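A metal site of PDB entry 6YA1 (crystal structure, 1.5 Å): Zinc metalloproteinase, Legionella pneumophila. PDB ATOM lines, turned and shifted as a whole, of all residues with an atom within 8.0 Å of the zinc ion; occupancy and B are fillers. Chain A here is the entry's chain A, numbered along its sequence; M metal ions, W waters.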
ATOM      1  N   ASP A  50     -13.855 -20.668   8.056  1.00  0.00           N
ATOM      2  CA  ASP A  50     -14.147 -21.959   7.443  1.00  0.00           C
ATOM      3  C   ASP A  50     -14.936 -21.714   6.164  1.00  0.00           C
ATOM      4  O   ASP A  50     -16.148 -21.407   6.200  1.00  0.00           O
ATOM      5  CB  ASP A  50     -14.892 -22.868   8.412  1.00  0.00           C
ATOM      6  CG  ASP A  50     -15.251 -24.210   7.812  1.00  0.00           C
ATOM      7  OD1 ASP A  50     -14.983 -24.454   6.602  1.00  0.00           O
ATOM      8  OD2 ASP A  50     -15.815 -25.034   8.574  1.00  0.00           O
ATOM      9  N   MET A  51     -14.253 -21.841   5.030  1.00  0.00           N
ATOM     10  CA  MET A  51     -14.894 -21.591   3.740  1.00  0.00           C
ATOM     11  C   MET A  51     -15.915 -22.651   3.366  1.00  0.00           C
ATOM     12  O   MET A  51     -16.671 -22.421   2.417  1.00  0.00           O
ATOM     13  CB  MET A  51     -13.836 -21.468   2.640  1.00  0.00           C
ATOM     14  CG  MET A  51     -12.824 -20.330   2.820  1.00  0.00           C
ATOM     15  SD  MET A  51     -13.520 -18.700   2.691  1.00  0.00           S
ATOM     16  CE  MET A  51     -14.062 -18.671   0.961  1.00  0.00           C
ATOM     17  N   GLY A  52     -15.976 -23.778   4.064  1.00  0.00           N
ATOM     18  CA  GLY A  52     -16.971 -24.786   3.749  1.00  0.00           C
ATOM     19  C   GLY A  52     -16.882 -25.265   2.321  1.00  0.00           C
ATOM     20  O   GLY A  52     -17.910 -25.620   1.717  1.00  0.00           O
ATOM     21  N   HIS A  53     -15.664 -25.284   1.773  1.00  0.00           N
ATOM     22  CA  HIS A  53     -15.364 -25.788   0.442  1.00  0.00           C
ATOM     23  C   HIS A  53     -15.949 -24.944  -0.668  1.00  0.00           C
ATOM     24  O   HIS A  53     -16.053 -25.413  -1.806  1.00  0.00           O
ATOM     25  CB  HIS A  53     -15.748 -27.240   0.313  1.00  0.00           C
ATOM     26  CG  HIS A  53     -15.156 -28.041   1.398  1.00  0.00           C
ATOM     27  ND1 HIS A  53     -15.906 -28.852   2.233  1.00  0.00           N
ATOM     28  CD2 HIS A  53     -13.910 -28.045   1.883  1.00  0.00           C
ATOM     29  CE1 HIS A  53     -15.107 -29.396   3.133  1.00  0.00           C
ATOM     30  NE2 HIS A  53     -13.889 -28.925   2.934  1.00  0.00           N
ATOM     31  N   ASP A  88     -11.126 -31.387  13.296  1.00  0.00           N
ATOM     32  CA  ASP A  88     -11.790 -30.805  12.133  1.00  0.00           C
ATOM     33  C   ASP A  88     -11.148 -31.521  10.952  1.00  0.00           C
ATOM     34  O   ASP A  88     -10.445 -30.950  10.132  1.00  0.00           O
ATOM     35  CB  ASP A  88     -11.580 -29.287  12.102  1.00  0.00           C
ATOM     36  CG  ASP A  88     -12.197 -28.629  10.882  1.00  0.00           C
ATOM     37  OD1 ASP A  88     -13.218 -29.122  10.364  1.00  0.00           O
ATOM     38  OD2 ASP A  88     -11.657 -27.600  10.434  1.00  0.00           O
ATOM     39  N   ARG A  89     -11.399 -32.830  10.868  1.00  0.00           N
ATOM     40  CA  ARG A  89     -10.605 -33.681  10.004  1.00  0.00           C
ATOM     41  C   ARG A  89     -10.864 -33.376   8.530  1.00  0.00           C
ATOM     42  O   ARG A  89     -11.986 -33.056   8.126  1.00  0.00           O
ATOM     43  CB  ARG A  89     -10.917 -35.153  10.291  1.00  0.00           C
ATOM     44  CG  ARG A  89     -10.545 -35.623  11.692  1.00  0.00           C
ATOM     45  CD  ARG A  89     -10.512 -37.144  11.742  1.00  0.00           C
ATOM     46  NE  ARG A  89      -9.925 -37.716  12.963  1.00  0.00           N
ATOM     47  CZ  ARG A  89      -8.628 -37.911  13.146  1.00  0.00           C
ATOM     48  NH1 ARG A  89      -7.752 -37.567  12.221  1.00  0.00           N
ATOM     49  NH2 ARG A  89      -8.193 -38.463  14.277  1.00  0.00           N
ATOM     50  N   ASP A  90      -9.806 -33.466   7.730  1.00  0.00           N
ATOM     51  CA  ASP A  90      -9.915 -33.173   6.316  1.00  0.00           C
ATOM     52  C   ASP A  90      -8.717 -33.720   5.569  1.00  0.00           C
ATOM     53  O   ASP A  90      -7.566 -33.379   5.877  1.00  0.00           O
ATOM     54  CB  ASP A  90     -10.048 -31.660   6.100  1.00  0.00           C
ATOM     55  CG  ASP A  90     -10.733 -31.350   4.820  1.00  0.00           C
ATOM     56  OD1 ASP A  90     -10.121 -31.720   3.793  1.00  0.00           O
ATOM     57  OD2 ASP A  90     -11.865 -30.792   4.833  1.00  0.00           O
ATOM     58  N   ASN A  91      -8.974 -34.553   4.565  1.00  0.00           N
ATOM     59  CA  ASN A  91      -7.948 -35.085   3.653  1.00  0.00           C
ATOM     60  C   ASN A  91      -6.653 -35.450   4.373  1.00  0.00           C
ATOM     61  O   ASN A  91      -5.548 -35.062   3.977  1.00  0.00           O
ATOM     62  CB  ASN A  91      -7.643 -34.076   2.551  1.00  0.00           C
ATOM     63  CG  ASN A  91      -6.764 -34.644   1.453  1.00  0.00           C
ATOM     64  OD1 ASN A  91      -6.766 -35.855   1.183  1.00  0.00           O
ATOM     65  ND2 ASN A  91      -6.009 -33.759   0.791  1.00  0.00           N
ATOM     66  N   PRO A  96      -7.194 -28.646   9.988  1.00  0.00           N
ATOM     67  CA  PRO A  96      -6.529 -27.508   9.315  1.00  0.00           C
ATOM     68  C   PRO A  96      -6.902 -26.176   9.938  1.00  0.00           C
ATOM     69  O   PRO A  96      -6.096 -25.234   9.881  1.00  0.00           O
ATOM     70  CB  PRO A  96      -6.992 -27.623   7.863  1.00  0.00           C
ATOM     71  CG  PRO A  96      -7.431 -29.094   7.706  1.00  0.00           C
ATOM     72  CD  PRO A  96      -7.958 -29.508   9.057  1.00  0.00           C
ATOM     73  N   THR A  97      -8.099 -26.048  10.522  1.00  0.00           N
ATOM     74  CA  THR A  97      -8.460 -24.779  11.139  1.00  0.00           C
ATOM     75  C   THR A  97      -7.644 -24.515  12.403  1.00  0.00           C
ATOM     76  O   THR A  97      -7.203 -23.380  12.622  1.00  0.00           O
ATOM     77  CB  THR A  97      -9.950 -24.736  11.430  1.00  0.00           C
ATOM     78  OG1 THR A  97     -10.358 -25.944  12.072  1.00  0.00           O
ATOM     79  CG2 THR A  97     -10.734 -24.574  10.130  1.00  0.00           C
ATOM     80  N   VAL A 134      -9.644 -21.134   5.357  1.00  0.00           N
ATOM     81  CA  VAL A 134      -9.317 -22.544   5.359  1.00  0.00           C
ATOM     82  C   VAL A 134     -10.499 -23.322   4.744  1.00  0.00           C
ATOM     83  O   VAL A 134     -11.599 -22.799   4.641  1.00  0.00           O
ATOM     84  CB  VAL A 134      -8.997 -23.020   6.796  1.00  0.00           C
ATOM     85  CG1 VAL A 134      -8.551 -24.463   6.815  1.00  0.00           C
ATOM     86  CG2 VAL A 134      -7.895 -22.128   7.404  1.00  0.00           C
ATOM     87  N   HIS A 135     -10.249 -24.565   4.345  1.00  0.00           N
ATOM     88  CA  HIS A 135     -11.263 -25.370   3.648  1.00  0.00           C
ATOM     89  C   HIS A 135     -11.707 -24.684   2.361  1.00  0.00           C
ATOM     90  O   HIS A 135     -12.877 -24.752   1.976  1.00  0.00           O
ATOM     91  CB  HIS A 135     -12.493 -25.655   4.536  1.00  0.00           C
ATOM     92  CG  HIS A 135     -12.175 -26.421   5.790  1.00  0.00           C
ATOM     93  ND1 HIS A 135     -11.876 -27.764   5.779  1.00  0.00           N
ATOM     94  CD2 HIS A 135     -12.158 -26.051   7.097  1.00  0.00           C
ATOM     95  CE1 HIS A 135     -11.623 -28.185   7.009  1.00  0.00           C
ATOM     96  NE2 HIS A 135     -11.813 -27.175   7.831  1.00  0.00           N
ATOM     97  N   TYR A 136     -10.787 -24.000   1.698  1.00  0.00           N
ATOM     98  CA  TYR A 136     -11.140 -23.257   0.497  1.00  0.00           C
ATOM     99  C   TYR A 136     -11.315 -24.185  -0.692  1.00  0.00           C
ATOM    100  O   TYR A 136     -10.422 -24.961  -1.009  1.00  0.00           O
ATOM    101  CB  TYR A 136     -10.021 -22.286   0.169  1.00  0.00           C
ATOM    102  CG  TYR A 136     -10.196 -21.456  -1.074  1.00  0.00           C
ATOM    103  CD1 TYR A 136     -11.001 -20.317  -1.075  1.00  0.00           C
ATOM    104  CD2 TYR A 136      -9.519 -21.790  -2.226  1.00  0.00           C
ATOM    105  CE1 TYR A 136     -11.101 -19.544  -2.214  1.00  0.00           C
ATOM    106  CE2 TYR A 136      -9.622 -21.034  -3.355  1.00  0.00           C
ATOM    107  CZ  TYR A 136     -10.408 -19.918  -3.349  1.00  0.00           C
ATOM    108  OH  TYR A 136     -10.483 -19.169  -4.503  1.00  0.00           O
ATOM    109  N   GLY A 137     -12.475 -24.114  -1.340  1.00  0.00           N
ATOM    110  CA  GLY A 137     -12.694 -24.877  -2.557  1.00  0.00           C
ATOM    111  C   GLY A 137     -12.835 -26.382  -2.323  1.00  0.00           C
ATOM    112  O   GLY A 137     -12.906 -26.870  -1.200  1.00  0.00           O
ATOM    113  N   GLN A 138     -12.925 -27.110  -3.442  1.00  0.00           N
ATOM    114  CA  GLN A 138     -13.048 -28.559  -3.430  1.00  0.00           C
ATOM    115  C   GLN A 138     -11.782 -29.135  -4.046  1.00  0.00           C
ATOM    116  O   GLN A 138     -11.527 -28.961  -5.239  1.00  0.00           O
ATOM    117  CB  GLN A 138     -14.267 -29.029  -4.208  1.00  0.00           C
ATOM    118  CG  GLN A 138     -15.572 -28.472  -3.677  1.00  0.00           C
ATOM    119  CD  GLN A 138     -16.740 -28.659  -4.638  1.00  0.00           C
ATOM    120  OE1 GLN A 138     -17.324 -29.736  -4.714  1.00  0.00           O
ATOM    121  NE2 GLN A 138     -17.074 -27.607  -5.373  1.00  0.00           N
ATOM    122  N   GLY A 139     -10.988 -29.838  -3.243  1.00  0.00           N
ATOM    123  CA  GLY A 139      -9.807 -30.469  -3.775  1.00  0.00           C
ATOM    124  C   GLY A 139      -8.791 -29.486  -4.294  1.00  0.00           C
ATOM    125  O   GLY A 139      -8.072 -29.777  -5.257  1.00  0.00           O
ATOM    126  N   PHE A 152      -6.157 -21.075   1.826  1.00  0.00           N
ATOM    127  CA  PHE A 152      -5.512 -22.368   1.878  1.00  0.00           C
ATOM    128  C   PHE A 152      -6.472 -23.482   1.469  1.00  0.00           C
ATOM    129  O   PHE A 152      -7.503 -23.698   2.128  1.00  0.00           O
ATOM    130  CB  PHE A 152      -4.953 -22.658   3.279  1.00  0.00           C
ATOM    131  CG  PHE A 152      -4.115 -21.552   3.865  1.00  0.00           C
ATOM    132  CD1 PHE A 152      -4.681 -20.518   4.582  1.00  0.00           C
ATOM    133  CD2 PHE A 152      -2.728 -21.551   3.723  1.00  0.00           C
ATOM    134  CE1 PHE A 152      -3.903 -19.486   5.124  1.00  0.00           C
ATOM    135  CE2 PHE A 152      -1.951 -20.527   4.270  1.00  0.00           C
ATOM    136  CZ  PHE A 152      -2.524 -19.512   4.973  1.00  0.00           C
ATOM    137  N   GLY A 153      -6.075 -24.244   0.467  1.00  0.00           N
ATOM    138  CA  GLY A 153      -6.843 -25.399   0.039  1.00  0.00           C
ATOM    139  C   GLY A 153      -6.669 -26.597   0.941  1.00  0.00           C
ATOM    140  O   GLY A 153      -5.808 -26.648   1.808  1.00  0.00           O
ATOM    141  N   ASP A 154      -7.554 -27.586   0.753  1.00  0.00           N
ATOM    142  CA  ASP A 154      -7.419 -28.835   1.495  1.00  0.00           C
ATOM    143  C   ASP A 154      -6.531 -29.840   0.775  1.00  0.00           C
ATOM    144  O   ASP A 154      -6.280 -30.916   1.322  1.00  0.00           O
ATOM    145  CB  ASP A 154      -8.781 -29.485   1.727  1.00  0.00           C
ATOM    146  CG  ASP A 154      -9.592 -28.787   2.765  1.00  0.00           C
ATOM    147  OD1 ASP A 154      -9.019 -28.225   3.708  1.00  0.00           O
ATOM    148  OD2 ASP A 154     -10.826 -28.818   2.653  1.00  0.00           O
ATOM    149  N   GLY A 155      -6.054 -29.525  -0.396  1.00  0.00           N
ATOM    150  CA  GLY A 155      -5.314 -30.495  -1.178  1.00  0.00           C
ATOM    151  C   GLY A 155      -6.203 -31.535  -1.805  1.00  0.00           C
ATOM    152  O   GLY A 155      -7.427 -31.519  -1.690  1.00  0.00           O
ATOM    153  N   PRO A 161      -3.924 -30.877   3.395  1.00  0.00           N
ATOM    154  CA  PRO A 161      -4.354 -29.479   3.505  1.00  0.00           C
ATOM    155  C   PRO A 161      -3.133 -28.575   3.680  1.00  0.00           C
ATOM    156  O   PRO A 161      -2.239 -28.865   4.462  1.00  0.00           O
ATOM    157  CB  PRO A 161      -5.270 -29.493   4.734  1.00  0.00           C
ATOM    158  CG  PRO A 161      -5.937 -30.910   4.650  1.00  0.00           C
ATOM    159  CD  PRO A 161      -4.793 -31.805   4.173  1.00  0.00           C
HETATM  160 ZN    ZN M   1     -12.119 -29.043   4.077  1.00  0.00          ZN
HETATM  161  O   HOH W   1     -11.738 -30.937   2.247  1.00  0.00           O
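OD2 of Asp 88 sits at hydrogen-bond distance from NE2 of His 135, at 2.6 Å. The backbone carbonyl oxygen (O) of Asp 154 sits at hydrogen-bond distance from the side-chain amide nitrogen (ND2) of Asn 91, at 2.9 Å.
The zinc ion is bound by the side-chain carboxylate of Asp 90 (1.9 Å), the side-chain carboxylate of Asp 154 (1.9 Å), a ring nitrogen (NE2) of His 53 (2.1 Å) and a ring nitrogen (ND1) of His 135 (2.1 Å). Slightly farther from the zinc ion lies water W1 (2.7 Å).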
